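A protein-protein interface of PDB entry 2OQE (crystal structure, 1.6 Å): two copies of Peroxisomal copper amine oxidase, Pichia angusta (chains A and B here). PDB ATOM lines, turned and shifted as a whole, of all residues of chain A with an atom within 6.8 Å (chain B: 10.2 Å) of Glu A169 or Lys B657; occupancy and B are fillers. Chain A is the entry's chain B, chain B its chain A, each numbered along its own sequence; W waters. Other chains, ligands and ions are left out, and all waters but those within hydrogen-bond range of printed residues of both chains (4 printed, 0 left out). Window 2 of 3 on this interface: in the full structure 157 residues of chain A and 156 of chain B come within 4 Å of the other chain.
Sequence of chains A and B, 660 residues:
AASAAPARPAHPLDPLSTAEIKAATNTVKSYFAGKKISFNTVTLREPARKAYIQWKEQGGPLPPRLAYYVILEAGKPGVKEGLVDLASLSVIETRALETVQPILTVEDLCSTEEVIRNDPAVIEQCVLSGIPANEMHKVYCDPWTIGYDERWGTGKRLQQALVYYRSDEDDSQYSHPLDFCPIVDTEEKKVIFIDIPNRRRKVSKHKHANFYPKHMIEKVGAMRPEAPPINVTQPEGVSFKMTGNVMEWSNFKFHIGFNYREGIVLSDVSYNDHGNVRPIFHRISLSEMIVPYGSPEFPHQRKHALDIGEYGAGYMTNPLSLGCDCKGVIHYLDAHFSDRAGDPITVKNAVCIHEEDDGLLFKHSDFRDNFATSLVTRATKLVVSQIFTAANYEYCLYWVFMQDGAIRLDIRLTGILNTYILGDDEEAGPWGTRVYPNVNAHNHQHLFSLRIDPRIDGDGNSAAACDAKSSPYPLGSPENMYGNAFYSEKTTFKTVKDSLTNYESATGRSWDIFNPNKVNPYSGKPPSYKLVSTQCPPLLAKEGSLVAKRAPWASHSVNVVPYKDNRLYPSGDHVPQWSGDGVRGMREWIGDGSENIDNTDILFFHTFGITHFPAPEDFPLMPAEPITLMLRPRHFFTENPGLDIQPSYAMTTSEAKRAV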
ATOM      1  N   TYR A 140     -10.922  -8.733  20.318  1.00  0.00           N
ATOM      2  CA  TYR A 140     -10.918 -10.165  20.059  1.00  0.00           C
ATOM      3  C   TYR A 140     -12.145 -10.504  19.246  1.00  0.00           C
ATOM      4  O   TYR A 140     -13.076  -9.692  19.164  1.00  0.00           O
ATOM      5  CB  TYR A 140     -10.952 -10.923  21.385  1.00  0.00           C
ATOM      6  CG  TYR A 140      -9.655 -10.823  22.176  1.00  0.00           C
ATOM      7  CD1 TYR A 140      -8.768 -11.903  22.223  1.00  0.00           C
ATOM      8  CD2 TYR A 140      -9.320  -9.662  22.868  1.00  0.00           C
ATOM      9  CE1 TYR A 140      -7.585 -11.824  22.954  1.00  0.00           C
ATOM     10  CE2 TYR A 140      -8.126  -9.575  23.595  1.00  0.00           C
ATOM     11  CZ  TYR A 140      -7.277 -10.654  23.636  1.00  0.00           C
ATOM     12  OH  TYR A 140      -6.100 -10.583  24.376  1.00  0.00           O
ATOM     13  N   ARG A 166     -11.385  -6.881  25.462  1.00  0.00           N
ATOM     14  CA  ARG A 166     -10.818  -7.212  26.766  1.00  0.00           C
ATOM     15  C   ARG A 166      -9.995  -6.032  27.261  1.00  0.00           C
ATOM     16  O   ARG A 166      -9.120  -5.527  26.532  1.00  0.00           O
ATOM     17  CB  ARG A 166      -9.910  -8.435  26.679  1.00  0.00           C
ATOM     18  CG  ARG A 166     -10.642  -9.724  26.317  1.00  0.00           C
ATOM     19  CD  ARG A 166      -9.710 -10.910  26.418  1.00  0.00           C
ATOM     20  NE  ARG A 166     -10.208 -12.064  25.665  1.00  0.00           N
ATOM     21  CZ  ARG A 166      -9.543 -13.211  25.516  1.00  0.00           C
ATOM     22  NH1 ARG A 166      -8.350 -13.377  26.089  1.00  0.00           N
ATOM     23  NH2 ARG A 166     -10.067 -14.199  24.799  1.00  0.00           N
ATOM     24  N   SER A 167     -10.259  -5.608  28.495  1.00  0.00           N
ATOM     25  CA  SER A 167      -9.443  -4.554  29.121  1.00  0.00           C
ATOM     26  C   SER A 167      -8.076  -5.108  29.539  1.00  0.00           C
ATOM     27  O   SER A 167      -7.090  -4.368  29.620  1.00  0.00           O
ATOM     28  CB  SER A 167     -10.170  -3.911  30.302  1.00  0.00           C
ATOM     29  OG  SER A 167     -10.196  -4.776  31.413  1.00  0.00           O
ATOM     30  N   ASP A 168      -8.029  -6.418  29.767  1.00  0.00           N
ATOM     31  CA  ASP A 168      -6.828  -7.131  30.153  1.00  0.00           C
ATOM     32  C   ASP A 168      -6.943  -8.534  29.562  1.00  0.00           C
ATOM     33  O   ASP A 168      -8.055  -9.049  29.438  1.00  0.00           O
ATOM     34  CB  ASP A 168      -6.750  -7.183  31.676  1.00  0.00           C
ATOM     35  CG  ASP A 168      -5.648  -8.081  32.167  1.00  0.00           C
ATOM     36  OD1 ASP A 168      -4.473  -7.658  32.129  1.00  0.00           O
ATOM     37  OD2 ASP A 168      -5.962  -9.209  32.590  1.00  0.00           O
ATOM     38  N   GLU A 169      -5.819  -9.137  29.173  1.00  0.00           N
ATOM     39  CA  GLU A 169      -5.844 -10.426  28.467  1.00  0.00           C
ATOM     40  C   GLU A 169      -6.548 -11.532  29.264  1.00  0.00           C
ATOM     41  O   GLU A 169      -7.039 -12.491  28.676  1.00  0.00           O
ATOM     42  CB  GLU A 169      -4.433 -10.888  28.062  1.00  0.00           C
ATOM     43  CG  GLU A 169      -3.532 -11.243  29.245  1.00  0.00           C
ATOM     44  CD  GLU A 169      -2.055 -11.418  28.887  1.00  0.00           C
ATOM     45  OE1 GLU A 169      -1.730 -11.729  27.722  1.00  0.00           O
ATOM     46  OE2 GLU A 169      -1.217 -11.249  29.797  1.00  0.00           O
ATOM     47  N   ASP A 170      -6.574 -11.391  30.587  1.00  0.00           N
ATOM     48  CA  ASP A 170      -7.169 -12.407  31.469  1.00  0.00           C
ATOM     49  C   ASP A 170      -8.672 -12.220  31.671  1.00  0.00           C
ATOM     50  O   ASP A 170      -9.317 -13.050  32.313  1.00  0.00           O
ATOM     51  CB  ASP A 170      -6.455 -12.431  32.820  1.00  0.00           C
ATOM     52  CG  ASP A 170      -5.040 -12.999  32.731  1.00  0.00           C
ATOM     53  OD1 ASP A 170      -4.665 -13.559  31.684  1.00  0.00           O
ATOM     54  OD2 ASP A 170      -4.308 -12.902  33.735  1.00  0.00           O
ATOM     55  N   ASP A 171      -9.225 -11.131  31.137  1.00  0.00           N
ATOM     56  CA  ASP A 171     -10.679 -10.904  31.177  1.00  0.00           C
ATOM     57  C   ASP A 171     -11.427 -11.976  30.417  1.00  0.00           C
ATOM     58  O   ASP A 171     -10.909 -12.540  29.464  1.00  0.00           O
ATOM     59  CB  ASP A 171     -11.047  -9.580  30.509  1.00  0.00           C
ATOM     60  CG  ASP A 171     -10.684  -8.378  31.340  1.00  0.00           C
ATOM     61  OD1 ASP A 171     -10.421  -8.517  32.558  1.00  0.00           O
ATOM     62  OD2 ASP A 171     -10.677  -7.275  30.762  1.00  0.00           O
ATOM     63  N   SER A 172     -12.663 -12.227  30.838  1.00  0.00           N
ATOM     64  CA  SER A 172     -13.629 -12.897  29.982  1.00  0.00           C
ATOM     65  C   SER A 172     -14.319 -11.822  29.144  1.00  0.00           C
ATOM     66  O   SER A 172     -14.939 -10.886  29.676  1.00  0.00           O
ATOM     67  CB  SER A 172     -14.653 -13.669  30.809  1.00  0.00           C
ATOM     68  OG  SER A 172     -15.513 -14.357  29.918  1.00  0.00           O
ATOM     69  N   ASP B 366     -10.268 -21.466  26.477  1.00  0.00           N
ATOM     70  CA  ASP B 366     -10.105 -20.567  25.340  1.00  0.00           C
ATOM     71  C   ASP B 366      -9.387 -21.269  24.166  1.00  0.00           C
ATOM     72  O   ASP B 366      -8.259 -21.722  24.328  1.00  0.00           O
ATOM     73  CB  ASP B 366      -9.339 -19.326  25.832  1.00  0.00           C
ATOM     74  CG  ASP B 366      -9.356 -18.170  24.833  1.00  0.00           C
ATOM     75  OD1 ASP B 366      -9.592 -18.413  23.623  1.00  0.00           O
ATOM     76  OD2 ASP B 366      -9.127 -17.022  25.276  1.00  0.00           O
ATOM     77  N   ARG B 368      -7.976 -20.032  21.720  1.00  0.00           N
ATOM     78  CA  ARG B 368      -6.889 -19.211  21.177  1.00  0.00           C
ATOM     79  C   ARG B 368      -5.495 -19.744  21.510  1.00  0.00           C
ATOM     80  O   ARG B 368      -4.566 -19.622  20.697  1.00  0.00           O
ATOM     81  CB  ARG B 368      -7.021 -17.755  21.630  1.00  0.00           C
ATOM     82  CG  ARG B 368      -8.216 -17.048  21.004  1.00  0.00           C
ATOM     83  CD  ARG B 368      -8.569 -15.733  21.710  1.00  0.00           C
ATOM     84  NE  ARG B 368      -9.789 -15.173  21.116  1.00  0.00           N
ATOM     85  CZ  ARG B 368     -11.026 -15.552  21.438  1.00  0.00           C
ATOM     86  NH1 ARG B 368     -11.235 -16.471  22.377  1.00  0.00           N
ATOM     87  NH2 ARG B 368     -12.061 -15.008  20.821  1.00  0.00           N
ATOM     88  N   ASP B 369      -5.359 -20.341  22.693  1.00  0.00           N
ATOM     89  CA  ASP B 369      -4.108 -21.010  23.070  1.00  0.00           C
ATOM     90  C   ASP B 369      -4.265 -22.526  23.223  1.00  0.00           C
ATOM     91  O   ASP B 369      -3.642 -23.138  24.095  1.00  0.00           O
ATOM     92  CB  ASP B 369      -3.492 -20.362  24.313  1.00  0.00           C
ATOM     93  CG  ASP B 369      -4.429 -20.357  25.519  1.00  0.00           C
ATOM     94  OD1 ASP B 369      -5.461 -21.082  25.519  1.00  0.00           O
ATOM     95  OD2 ASP B 369      -4.118 -19.623  26.482  1.00  0.00           O
ATOM     96  N   PHE B 371      -6.724 -24.216  24.319  1.00  0.00           N
ATOM     97  CA  PHE B 371      -7.395 -24.570  25.574  1.00  0.00           C
ATOM     98  C   PHE B 371      -6.471 -24.602  26.792  1.00  0.00           C
ATOM     99  O   PHE B 371      -6.828 -25.160  27.838  1.00  0.00           O
ATOM    100  CB  PHE B 371      -8.163 -25.893  25.420  1.00  0.00           C
ATOM    101  CG  PHE B 371      -9.103 -25.911  24.256  1.00  0.00           C
ATOM    102  CD1 PHE B 371     -10.058 -24.909  24.097  1.00  0.00           C
ATOM    103  CD2 PHE B 371      -9.048 -26.932  23.318  1.00  0.00           C
ATOM    104  CE1 PHE B 371     -10.937 -24.922  23.015  1.00  0.00           C
ATOM    105  CE2 PHE B 371      -9.924 -26.950  22.234  1.00  0.00           C
ATOM    106  CZ  PHE B 371     -10.869 -25.940  22.078  1.00  0.00           C
ATOM    107  N   ALA B 372      -5.287 -24.000  26.666  1.00  0.00           N
ATOM    108  CA  ALA B 372      -4.387 -23.840  27.809  1.00  0.00           C
ATOM    109  C   ALA B 372      -4.986 -22.896  28.846  1.00  0.00           C
ATOM    110  O   ALA B 372      -4.826 -23.111  30.059  1.00  0.00           O
ATOM    111  CB  ALA B 372      -3.025 -23.339  27.367  1.00  0.00           C
ATOM    112  N   THR B 373      -5.659 -21.847  28.371  1.00  0.00           N
ATOM    113  CA  THR B 373      -6.463 -20.993  29.238  1.00  0.00           C
ATOM    114  C   THR B 373      -7.737 -21.768  29.576  1.00  0.00           C
ATOM    115  O   THR B 373      -8.522 -22.107  28.688  1.00  0.00           O
ATOM    116  CB  THR B 373      -6.833 -19.661  28.549  1.00  0.00           C
ATOM    117  OG1 THR B 373      -5.645 -18.884  28.349  1.00  0.00           O
ATOM    118  CG2 THR B 373      -7.799 -18.854  29.412  1.00  0.00           C
ATOM    119  N   SER B 374      -7.914 -22.081  30.854  1.00  0.00           N
ATOM    120  CA  SER B 374      -8.968 -23.014  31.254  1.00  0.00           C
ATOM    121  C   SER B 374      -9.306 -22.914  32.727  1.00  0.00           C
ATOM    122  O   SER B 374      -8.427 -22.697  33.567  1.00  0.00           O
ATOM    123  CB  SER B 374      -8.541 -24.450  30.931  1.00  0.00           C
ATOM    124  OG  SER B 374      -9.616 -25.347  31.113  1.00  0.00           O
ATOM    125  N   TYR B 649      -9.094 -26.884  38.689  1.00  0.00           N
ATOM    126  CA  TYR B 649      -7.961 -26.430  37.890  1.00  0.00           C
ATOM    127  C   TYR B 649      -8.262 -25.059  37.321  1.00  0.00           C
ATOM    128  O   TYR B 649      -9.367 -24.817  36.846  1.00  0.00           O
ATOM    129  CB  TYR B 649      -7.665 -27.396  36.751  1.00  0.00           C
ATOM    130  CG  TYR B 649      -6.487 -26.965  35.895  1.00  0.00           C
ATOM    131  CD1 TYR B 649      -5.181 -27.113  36.365  1.00  0.00           C
ATOM    132  CD2 TYR B 649      -6.673 -26.417  34.629  1.00  0.00           C
ATOM    133  CE1 TYR B 649      -4.087 -26.729  35.590  1.00  0.00           C
ATOM    134  CE2 TYR B 649      -5.586 -26.022  33.845  1.00  0.00           C
ATOM    135  CZ  TYR B 649      -4.296 -26.185  34.336  1.00  0.00           C
ATOM    136  OH  TYR B 649      -3.208 -25.807  33.579  1.00  0.00           O
ATOM    137  N   MET B 651      -6.111 -21.949  34.965  1.00  0.00           N
ATOM    138  CA  MET B 651      -4.965 -21.305  34.349  1.00  0.00           C
ATOM    139  C   MET B 651      -5.468 -20.155  33.498  1.00  0.00           C
ATOM    140  O   MET B 651      -6.324 -20.328  32.622  1.00  0.00           O
ATOM    141  CB  MET B 651      -4.145 -22.283  33.506  1.00  0.00           C
ATOM    142  CG  MET B 651      -3.015 -21.602  32.722  1.00  0.00           C
ATOM    143  SD  MET B 651      -1.832 -22.722  31.944  1.00  0.00           S
ATOM    144  CE  MET B 651      -0.820 -23.187  33.342  1.00  0.00           C
ATOM    145  N   THR B 652      -4.955 -18.963  33.794  1.00  0.00           N
ATOM    146  CA  THR B 652      -5.317 -17.774  33.038  1.00  0.00           C
ATOM    147  C   THR B 652      -4.473 -17.671  31.766  1.00  0.00           C
ATOM    148  O   THR B 652      -3.495 -18.412  31.591  1.00  0.00           O
ATOM    149  CB  THR B 652      -5.088 -16.494  33.849  1.00  0.00           C
ATOM    150  OG1 THR B 652      -3.698 -16.388  34.149  1.00  0.00           O
ATOM    151  CG2 THR B 652      -5.870 -16.495  35.153  1.00  0.00           C
ATOM    152  N   THR B 653      -4.835 -16.727  30.892  1.00  0.00           N
ATOM    153  CA  THR B 653      -4.090 -16.517  29.652  1.00  0.00           C
ATOM    154  C   THR B 653      -2.644 -16.095  29.923  1.00  0.00           C
ATOM    155  O   THR B 653      -1.727 -16.627  29.297  1.00  0.00           O
ATOM    156  CB  THR B 653      -4.817 -15.541  28.702  1.00  0.00           C
ATOM    157  OG1 THR B 653      -6.006 -16.175  28.221  1.00  0.00           O
ATOM    158  CG2 THR B 653      -3.948 -15.183  27.485  1.00  0.00           C
ATOM    159  N   SER B 654      -2.456 -15.168  30.861  1.00  0.00           N
ATOM    160  CA  SER B 654      -1.119 -14.697  31.209  1.00  0.00           C
ATOM    161  C   SER B 654      -0.273 -15.821  31.807  1.00  0.00           C
ATOM    162  O   SER B 654       0.903 -15.975  31.454  1.00  0.00           O
ATOM    163  CB  SER B 654      -1.182 -13.493  32.153  1.00  0.00           C
ATOM    164  OG  SER B 654      -1.790 -13.816  33.391  1.00  0.00           O
ATOM    165  N   GLU B 655      -0.875 -16.616  32.690  1.00  0.00           N
ATOM    166  CA  GLU B 655      -0.185 -17.767  33.272  1.00  0.00           C
ATOM    167  C   GLU B 655       0.209 -18.781  32.194  1.00  0.00           C
ATOM    168  O   GLU B 655       1.314 -19.332  32.224  1.00  0.00           O
ATOM    169  CB  GLU B 655      -1.046 -18.438  34.346  1.00  0.00           C
ATOM    170  CG  GLU B 655      -1.176 -17.665  35.650  1.00  0.00           C
ATOM    171  CD  GLU B 655      -2.213 -18.274  36.589  1.00  0.00           C
ATOM    172  OE1 GLU B 655      -3.109 -19.029  36.122  1.00  0.00           O
ATOM    173  OE2 GLU B 655      -2.136 -17.992  37.807  1.00  0.00           O
ATOM    174  N   ALA B 656      -0.688 -19.025  31.238  1.00  0.00           N
ATOM    175  CA  ALA B 656      -0.392 -19.935  30.134  1.00  0.00           C
ATOM    176  C   ALA B 656       0.804 -19.452  29.302  1.00  0.00           C
ATOM    177  O   ALA B 656       1.634 -20.257  28.876  1.00  0.00           O
ATOM    178  CB  ALA B 656      -1.623 -20.148  29.248  1.00  0.00           C
ATOM    179  N   LYS B 657       0.885 -18.138  29.089  1.00  0.00           N
ATOM    180  CA  LYS B 657       1.973 -17.535  28.318  1.00  0.00           C
ATOM    181  C   LYS B 657       3.307 -17.644  29.051  1.00  0.00           C
ATOM    182  O   LYS B 657       4.323 -17.988  28.442  1.00  0.00           O
ATOM    183  CB  LYS B 657       1.670 -16.065  27.998  1.00  0.00           C
ATOM    184  CG  LYS B 657       0.661 -15.852  26.877  1.00  0.00           C
ATOM    185  CD  LYS B 657       0.568 -14.377  26.494  1.00  0.00           C
ATOM    186  CE  LYS B 657      -0.226 -14.193  25.198  1.00  0.00           C
ATOM    187  NZ  LYS B 657      -0.167 -12.796  24.659  1.00  0.00           N
ATOM    188  N   ARG B 658       3.307 -17.355  30.351  1.00  0.00           N
ATOM    189  CA  ARG B 658       4.553 -17.339  31.122  1.00  0.00           C
ATOM    190  C   ARG B 658       5.005 -18.740  31.562  1.00  0.00           C
ATOM    191  O   ARG B 658       6.094 -18.905  32.125  1.00  0.00           O
ATOM    192  CB  ARG B 658       4.497 -16.323  32.278  1.00  0.00           C
ATOM    193  CG  ARG B 658       4.090 -16.858  33.635  1.00  0.00           C
ATOM    194  CD  ARG B 658       4.158 -15.757  34.680  1.00  0.00           C
ATOM    195  NE  ARG B 658       2.968 -14.906  34.654  1.00  0.00           N
ATOM    196  CZ  ARG B 658       1.894 -15.087  35.422  1.00  0.00           C
ATOM    197  NH1 ARG B 658       1.847 -16.095  36.292  1.00  0.00           N
ATOM    198  NH2 ARG B 658       0.859 -14.258  35.323  1.00  0.00           N
ATOM    199  N   ALA B 659       4.166 -19.738  31.283  1.00  0.00           N
ATOM    200  CA  ALA B 659       4.549 -21.142  31.405  1.00  0.00           C
ATOM    201  C   ALA B 659       5.380 -21.575  30.191  1.00  0.00           C
ATOM    202  O   ALA B 659       5.826 -22.724  30.116  1.00  0.00           O
ATOM    203  CB  ALA B 659       3.315 -22.025  31.556  1.00  0.00           C
ATOM    204  N   VAL B 660       5.581 -20.641  29.257  1.00  0.00           N
ATOM    205  CA  VAL B 660       6.419 -20.819  28.049  1.00  0.00           C
ATOM    206  C   VAL B 660       6.334 -22.212  27.418  1.00  0.00           C
ATOM    207  O   VAL B 660       7.342 -22.833  27.037  1.00  0.00           O
ATOM    208  CB  VAL B 660       7.918 -20.376  28.262  1.00  0.00           C
ATOM    209  CG1 VAL B 660       8.016 -18.860  28.445  1.00  0.00           C
ATOM    210  CG2 VAL B 660       8.592 -21.131  29.430  1.00  0.00           C
ATOM    211  OXT VAL B 660       5.225 -22.740  27.280  1.00  0.00           O
HETATM  212  O   HOH W   1     -10.353 -16.200  27.586  1.00  0.00           O
HETATM  213  O   HOH W   2      -6.844 -15.968  25.723  1.00  0.00           O
HETATM  214  O   HOH W   3      -8.800 -14.685  29.232  1.00  0.00           O
HETATM  215  O   HOH W   4      -7.610 -15.957  31.493  1.00  0.00           O
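The side-chain hydroxyl of Ser B654 sits at hydrogen-bond distance from the side-chain carboxylate of Asp A170 (2.7 Å).
The side-chain carboxylate (OE1) of Glu A169 is in salt-bridge range of the side-chain amino group (NZ) of Lys B657 (3.6 Å).
N of Thr B653 is in hydrogen-bond range of OD1 of Asp A170, 3.3 Å away.
The side-chain carboxylate (OD2) of Asp B366 lies within salt-bridge range of the guanidinium group (NH2) of Arg A166, 3.0 Å away.
OG of Ser B654 lies within hydrogen-bond range of OG1 of Thr B652, 3.3 Å away.
N of Asp B366 lies within hydrogen-bond range of O of Thr B373 (2.9 Å).
The side-chain hydroxyl (OG1) of Thr B373 sits at hydrogen-bond distance from the side-chain hydroxyl (OG1) of Thr B653.
The side-chain carboxylate of Asp A168 lies within hydrogen-bond range of the backbone NH of Asp A170 (3.0 Å).
OD1 of Asp B366 lies within salt-bridge range of NH1 of Arg B368.
The guanidinium group of Arg B658 lies within hydrogen-bond range of the side-chain hydroxyl of Ser B654, at 3.3 Å.
Tyr A140 touches Arg B368.
NH2 of Arg A166 touches NH1 of Arg B368 (3.5 Å).
Thr B653 touches Glu A169 (CB to O, 3.8 Å).
CB of Ser B654 touches OE2 of Glu A169, 3.3 Å away.
Asp A170 touches Thr B652.
Printed residues of chain B within 4 Å of Tyr A140: Arg B368.
Asp A168 touches none of the printed residues of chain B.
Of the printed residues of chain B, Glu A169 touches Thr B653 (3.8 Å), Ser B654 (3.3 Å) and Lys B657 (3.6 Å).
No residue of chain B comes within 4 Å of Asp A171.
Printed residues of chain A within 4 Å of Asp B366: Arg A166.
Thr B373 touches none of the printed residues of chain A.
Of the printed residues of chain A, Thr B652 touches Asp A170.
Glu B655 touches none of the printed residues of chain A.
The nearest printed residue of chain B that does not touch Tyr A140 is Asp B366 (5.9 Å).
Printed residues of chain B that touch a printed residue of chain A: Asp B366, Arg B368, Thr B652, Thr B653, Ser B654 and Lys B657.
Among the printed residues, 9 pairs touch across the chains.
Among the printed residues, Asp or Glu carboxylates within 4 Å of a Lys or Arg side-chain nitrogen of the other chain: Arg A166 with Asp B366 (3.0 Å) and Glu A169 with Lys B657 (3.6 Å).
No position is printed for both chains.
Water W2 lies within hydrogen-bond range of OD2 of Asp B366 (2.6 Å), OG1 of Thr B653 (2.6 Å) and NH1 of Arg A166 (3.0 Å).
Water W1 bridges OD2 of Asp B366 (2.7 Å) and NH2 of Arg A166 (3.4 Å).
Water W3 lies within hydrogen-bond range of the backbone carbonyl oxygen of Glu A169 (2.9 Å), the backbone carbonyl oxygen of Asp A171 (3.0 Å), the side-chain hydroxyl of Thr B653 (3.3 Å) and the guanidinium group of Arg A166 (3.4 Å).
Water W4 bridges the backbone NH (N) of Thr B653 (2.9 Å) and the backbone carbonyl oxygen (O) of Asp A170 (3.5 Å).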
